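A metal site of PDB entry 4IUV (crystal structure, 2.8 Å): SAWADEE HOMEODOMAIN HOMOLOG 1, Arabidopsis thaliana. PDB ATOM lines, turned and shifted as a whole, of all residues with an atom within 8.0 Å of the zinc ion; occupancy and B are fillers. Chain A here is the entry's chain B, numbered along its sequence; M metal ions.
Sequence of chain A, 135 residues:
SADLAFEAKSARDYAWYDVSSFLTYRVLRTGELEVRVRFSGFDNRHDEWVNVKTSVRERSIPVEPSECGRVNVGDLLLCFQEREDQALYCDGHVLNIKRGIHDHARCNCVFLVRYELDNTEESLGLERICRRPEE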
ATOM      1  N   VAL A  63      -6.865  20.241   5.432  1.00  0.00           N
ATOM      2  CA  VAL A  63      -5.788  19.446   6.005  1.00  0.00           C
ATOM      3  C   VAL A  63      -6.115  19.042   7.439  1.00  0.00           C
ATOM      4  O   VAL A  63      -6.473  19.882   8.263  1.00  0.00           O
ATOM      5  CB  VAL A  63      -4.451  20.214   5.968  1.00  0.00           C
ATOM      6  CG1 VAL A  63      -3.292  19.251   6.177  1.00  0.00           C
ATOM      7  CG2 VAL A  63      -4.300  20.949   4.648  1.00  0.00           C
ATOM      8  N   GLU A  64      -5.981  17.753   7.735  1.00  0.00           N
ATOM      9  CA  GLU A  64      -6.268  17.227   9.067  1.00  0.00           C
ATOM     10  C   GLU A  64      -5.018  17.313   9.943  1.00  0.00           C
ATOM     11  O   GLU A  64      -3.914  17.074   9.461  1.00  0.00           O
ATOM     12  CB  GLU A  64      -6.768  15.786   8.974  1.00  0.00           C
ATOM     13  CG  GLU A  64      -7.180  15.147  10.292  1.00  0.00           C
ATOM     14  CD  GLU A  64      -8.689  15.133  10.498  1.00  0.00           C
ATOM     15  OE1 GLU A  64      -9.426  15.270   9.509  1.00  0.00           O
ATOM     16  OE2 GLU A  64      -9.125  14.986  11.661  1.00  0.00           O
ATOM     17  N   PRO A  65      -5.196  17.644  11.232  1.00  0.00           N
ATOM     18  CA  PRO A  65      -4.086  17.818  12.169  1.00  0.00           C
ATOM     19  C   PRO A  65      -2.987  16.766  12.037  1.00  0.00           C
ATOM     20  O   PRO A  65      -1.804  17.092  12.131  1.00  0.00           O
ATOM     21  CB  PRO A  65      -4.757  17.684  13.536  1.00  0.00           C
ATOM     22  CG  PRO A  65      -6.124  18.236  13.306  1.00  0.00           C
ATOM     23  CD  PRO A  65      -6.498  17.857  11.890  1.00  0.00           C
ATOM     24  N   SER A  66      -3.373  15.513  11.823  1.00  0.00           N
ATOM     25  CA  SER A  66      -2.407  14.433  11.662  1.00  0.00           C
ATOM     26  C   SER A  66      -1.688  14.483  10.299  1.00  0.00           C
ATOM     27  O   SER A  66      -0.790  13.684  10.036  1.00  0.00           O
ATOM     28  CB  SER A  66      -3.074  13.068  11.860  1.00  0.00           C
ATOM     29  OG  SER A  66      -4.337  13.014  11.219  1.00  0.00           O
ATOM     30  N   GLU A  67      -2.090  15.431   9.452  1.00  0.00           N
ATOM     31  CA  GLU A  67      -1.512  15.575   8.119  1.00  0.00           C
ATOM     32  C   GLU A  67      -0.503  16.714   8.009  1.00  0.00           C
ATOM     33  O   GLU A  67       0.319  16.734   7.093  1.00  0.00           O
ATOM     34  CB  GLU A  67      -2.612  15.820   7.085  1.00  0.00           C
ATOM     35  CG  GLU A  67      -3.488  14.627   6.764  1.00  0.00           C
ATOM     36  CD  GLU A  67      -4.622  14.988   5.828  1.00  0.00           C
ATOM     37  OE1 GLU A  67      -4.476  15.977   5.070  1.00  0.00           O
ATOM     38  OE2 GLU A  67      -5.658  14.294   5.841  1.00  0.00           O
ATOM     39  N   CYS A  68      -0.575  17.658   8.941  1.00  0.00           N
ATOM     40  CA  CYS A  68       0.168  18.912   8.840  1.00  0.00           C
ATOM     41  C   CYS A  68       1.616  18.755   8.380  1.00  0.00           C
ATOM     42  O   CYS A  68       2.247  19.722   7.943  1.00  0.00           O
ATOM     43  CB  CYS A  68       0.138  19.659  10.171  1.00  0.00           C
ATOM     44  SG  CYS A  68       1.135  18.856  11.450  1.00  0.00           S
ATOM     45  N   GLY A  69       2.159  17.556   8.500  1.00  0.00           N
ATOM     46  CA  GLY A  69       3.515  17.302   8.070  1.00  0.00           C
ATOM     47  C   GLY A  69       3.646  17.422   6.567  1.00  0.00           C
ATOM     48  O   GLY A  69       4.738  17.694   6.048  1.00  0.00           O
ATOM     49  N   ILE A  97       7.369  27.973   8.685  1.00  0.00           N
ATOM     50  CA  ILE A  97       6.485  27.203   9.563  1.00  0.00           C
ATOM     51  C   ILE A  97       7.065  27.025  10.971  1.00  0.00           C
ATOM     52  O   ILE A  97       8.197  26.576  11.137  1.00  0.00           O
ATOM     53  CB  ILE A  97       6.170  25.806   9.000  1.00  0.00           C
ATOM     54  CG1 ILE A  97       5.936  25.868   7.480  1.00  0.00           C
ATOM     55  CG2 ILE A  97       4.973  25.194   9.705  1.00  0.00           C
ATOM     56  CD1 ILE A  97       5.632  24.526   6.858  1.00  0.00           C
ATOM     57  N   LYS A  98       6.279  27.390  11.972  1.00  0.00           N
ATOM     58  CA  LYS A  98       6.612  27.086  13.351  1.00  0.00           C
ATOM     59  C   LYS A  98       5.804  25.879  13.791  1.00  0.00           C
ATOM     60  O   LYS A  98       4.587  25.951  13.947  1.00  0.00           O
ATOM     61  CB  LYS A  98       6.305  28.277  14.263  1.00  0.00           C
ATOM     62  CG  LYS A  98       7.163  29.498  13.997  1.00  0.00           C
ATOM     63  CD  LYS A  98       6.531  30.740  14.609  1.00  0.00           C
ATOM     64  CE  LYS A  98       7.183  32.019  14.125  1.00  0.00           C
ATOM     65  NZ  LYS A  98       8.180  32.554  15.090  1.00  0.00           N
ATOM     66  N   ARG A  99       6.486  24.744  13.965  1.00  0.00           N
ATOM     67  CA  ARG A  99       5.828  23.512  14.358  1.00  0.00           C
ATOM     68  C   ARG A  99       5.560  23.485  15.855  1.00  0.00           C
ATOM     69  O   ARG A  99       6.434  23.831  16.657  1.00  0.00           O
ATOM     70  CB  ARG A  99       6.680  22.303  13.945  1.00  0.00           C
ATOM     71  CG  ARG A  99       6.862  22.156  12.441  1.00  0.00           C
ATOM     72  CD  ARG A  99       5.573  21.687  11.767  1.00  0.00           C
ATOM     73  NE  ARG A  99       5.696  21.629  10.321  1.00  0.00           N
ATOM     74  CZ  ARG A  99       4.716  21.253   9.504  1.00  0.00           C
ATOM     75  NH1 ARG A  99       3.529  20.908   9.997  1.00  0.00           N
ATOM     76  NH2 ARG A  99       4.909  21.221   8.198  1.00  0.00           N
ATOM     77  N   GLY A 100       4.348  23.093  16.231  1.00  0.00           N
ATOM     78  CA  GLY A 100       3.970  23.019  17.626  1.00  0.00           C
ATOM     79  C   GLY A 100       3.844  21.577  18.102  1.00  0.00           C
ATOM     80  O   GLY A 100       4.082  20.655  17.335  1.00  0.00           O
ATOM     81  N   ILE A 101       3.450  21.404  19.354  1.00  0.00           N
ATOM     82  CA  ILE A 101       3.194  20.083  19.903  1.00  0.00           C
ATOM     83  C   ILE A 101       1.698  19.866  20.058  1.00  0.00           C
ATOM     84  O   ILE A 101       1.039  20.530  20.871  1.00  0.00           O
ATOM     85  CB  ILE A 101       3.881  19.896  21.272  1.00  0.00           C
ATOM     86  CG1 ILE A 101       4.951  20.961  21.487  1.00  0.00           C
ATOM     87  CG2 ILE A 101       4.335  18.414  21.461  1.00  0.00           C
ATOM     88  CD1 ILE A 101       5.198  21.342  22.943  1.00  0.00           C
ATOM     89  N   HIS A 102       1.157  18.939  19.276  1.00  0.00           N
ATOM     90  CA  HIS A 102      -0.265  18.667  19.326  1.00  0.00           C
ATOM     91  C   HIS A 102      -0.521  17.240  18.857  1.00  0.00           C
ATOM     92  O   HIS A 102       0.354  16.592  18.281  1.00  0.00           O
ATOM     93  CB  HIS A 102      -1.021  19.652  18.433  1.00  0.00           C
ATOM     94  CG  HIS A 102      -0.597  19.588  17.007  1.00  0.00           C
ATOM     95  ND1 HIS A 102      -1.030  18.612  16.135  1.00  0.00           N
ATOM     96  CD2 HIS A 102       0.251  20.379  16.285  1.00  0.00           C
ATOM     97  CE1 HIS A 102      -0.484  18.805  14.948  1.00  0.00           C
ATOM     98  NE2 HIS A 102       0.292  19.869  15.013  1.00  0.00           N
ATOM     99  N   ASP A 103      -1.732  16.770  19.105  1.00  0.00           N
ATOM    100  CA  ASP A 103      -2.109  15.424  18.710  1.00  0.00           C
ATOM    101  C   ASP A 103      -2.886  15.449  17.396  1.00  0.00           C
ATOM    102  O   ASP A 103      -2.655  16.295  16.536  1.00  0.00           O
ATOM    103  CB  ASP A 103      -2.946  14.771  19.810  1.00  0.00           C
ATOM    104  CG  ASP A 103      -4.195  15.562  20.133  1.00  0.00           C
ATOM    105  OD1 ASP A 103      -4.288  16.731  19.713  1.00  0.00           O
ATOM    106  OD2 ASP A 103      -5.090  15.021  20.822  1.00  0.00           O
ATOM    107  N   ARG A 106      -6.133  18.744  16.998  1.00  0.00           N
ATOM    108  CA  ARG A 106      -6.042  20.145  16.571  1.00  0.00           C
ATOM    109  C   ARG A 106      -4.595  20.505  16.291  1.00  0.00           C
ATOM    110  O   ARG A 106      -3.692  20.137  17.043  1.00  0.00           O
ATOM    111  CB  ARG A 106      -6.615  21.057  17.653  1.00  0.00           C
ATOM    112  CG  ARG A 106      -6.460  22.545  17.406  1.00  0.00           C
ATOM    113  CD  ARG A 106      -7.699  23.152  16.785  1.00  0.00           C
ATOM    114  NE  ARG A 106      -7.644  24.616  16.797  1.00  0.00           N
ATOM    115  CZ  ARG A 106      -8.600  25.401  16.308  1.00  0.00           C
ATOM    116  NH1 ARG A 106      -8.455  26.716  16.360  1.00  0.00           N
ATOM    117  NH2 ARG A 106      -9.675  24.874  15.758  1.00  0.00           N
ATOM    118  N   CYS A 107      -4.357  21.224  15.187  1.00  0.00           N
ATOM    119  CA  CYS A 107      -3.000  21.592  14.801  1.00  0.00           C
ATOM    120  C   CYS A 107      -2.651  23.014  15.206  1.00  0.00           C
ATOM    121  O   CYS A 107      -3.219  23.973  14.677  1.00  0.00           O
ATOM    122  CB  CYS A 107      -2.817  21.415  13.295  1.00  0.00           C
ATOM    123  SG  CYS A 107      -1.425  22.348  12.608  1.00  0.00           S
ATOM    124  N   ASN A 108      -1.719  23.160  16.139  1.00  0.00           N
ATOM    125  CA  ASN A 108      -1.295  24.480  16.588  1.00  0.00           C
ATOM    126  C   ASN A 108       0.010  24.951  15.934  1.00  0.00           C
ATOM    127  O   ASN A 108       0.635  25.896  16.402  1.00  0.00           O
ATOM    128  CB  ASN A 108      -1.166  24.534  18.114  1.00  0.00           C
ATOM    129  CG  ASN A 108      -0.199  23.489  18.664  1.00  0.00           C
ATOM    130  OD1 ASN A 108       0.628  22.943  17.933  1.00  0.00           O
ATOM    131  ND2 ASN A 108      -0.306  23.218  19.954  1.00  0.00           N
ATOM    132  N   CYS A 109       0.395  24.293  14.842  1.00  0.00           N
ATOM    133  CA  CYS A 109       1.509  24.754  14.037  1.00  0.00           C
ATOM    134  C   CYS A 109       1.122  26.082  13.381  1.00  0.00           C
ATOM    135  O   CYS A 109      -0.043  26.303  13.052  1.00  0.00           O
ATOM    136  CB  CYS A 109       1.877  23.722  12.974  1.00  0.00           C
ATOM    137  SG  CYS A 109       2.452  22.141  13.640  1.00  0.00           S
ATOM    138  N   VAL A 110       2.099  26.965  13.210  1.00  0.00           N
ATOM    139  CA  VAL A 110       1.823  28.293  12.657  1.00  0.00           C
ATOM    140  C   VAL A 110       2.464  28.490  11.294  1.00  0.00           C
ATOM    141  O   VAL A 110       3.660  28.248  11.125  1.00  0.00           O
ATOM    142  CB  VAL A 110       2.271  29.406  13.620  1.00  0.00           C
ATOM    143  CG1 VAL A 110       2.342  30.743  12.896  1.00  0.00           C
ATOM    144  CG2 VAL A 110       1.328  29.487  14.814  1.00  0.00           C
ATOM    145  N   PHE A 111       1.668  28.929  10.335  1.00  0.00           N
ATOM    146  CA  PHE A 111       2.121  29.082   8.954  1.00  0.00           C
ATOM    147  C   PHE A 111       2.187  30.540   8.525  1.00  0.00           C
ATOM    148  O   PHE A 111       1.168  31.225   8.466  1.00  0.00           O
ATOM    149  CB  PHE A 111       1.202  28.309   8.004  1.00  0.00           C
ATOM    150  CG  PHE A 111       1.078  26.851   8.336  1.00  0.00           C
ATOM    151  CD1 PHE A 111       1.791  25.905   7.628  1.00  0.00           C
ATOM    152  CD2 PHE A 111       0.244  26.428   9.369  1.00  0.00           C
ATOM    153  CE1 PHE A 111       1.677  24.560   7.929  1.00  0.00           C
ATOM    154  CE2 PHE A 111       0.131  25.096   9.675  1.00  0.00           C
ATOM    155  CZ  PHE A 111       0.841  24.154   8.959  1.00  0.00           C
ATOM    156  N   LEU A 126      -3.598  25.799  10.684  1.00  0.00           N
ATOM    157  CA  LEU A 126      -4.036  24.779   9.737  1.00  0.00           C
ATOM    158  C   LEU A 126      -5.537  24.884   9.482  1.00  0.00           C
ATOM    159  O   LEU A 126      -6.029  24.442   8.438  1.00  0.00           O
ATOM    160  CB  LEU A 126      -3.720  23.379  10.269  1.00  0.00           C
ATOM    161  CG  LEU A 126      -3.857  22.243   9.256  1.00  0.00           C
ATOM    162  CD1 LEU A 126      -2.651  22.225   8.341  1.00  0.00           C
ATOM    163  CD2 LEU A 126      -3.992  20.903   9.965  1.00  0.00           C
HETATM  164 ZN    ZN M   1       0.431  20.687  12.958  1.00  0.00          ZN
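NE2 of His 102 is bound to the zinc ion (2.2 Å). The zinc ion is bound by SG of Cys 68 (2.5 Å). The zinc ion is bound by the side-chain sulfur (SG) of Cys 107 (2.5 Å). The zinc ion is bound by the side-chain sulfur (SG) of Cys 109, 2.6 Å away. The zinc ion has four donor atoms within binding distance.
The backbone NH (N) of Gly 100 sits close to the side-chain sulfur (SG) of Cys 109, at 3.3 Å. SG of Cys 68 lies close to O of Pro 65, at 3.5 Å. The backbone carbonyl oxygen (O) of Cys 68 lies within hydrogen-bond range of the guanidinium group (NH1) of Arg 99 (2.7 Å). ND1 of His 102 lies close to O of Arg 106, at 3.2 Å.
Within 4 Å of the zinc ion: Cys 68, His 102, Cys 107 and Cys 109.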
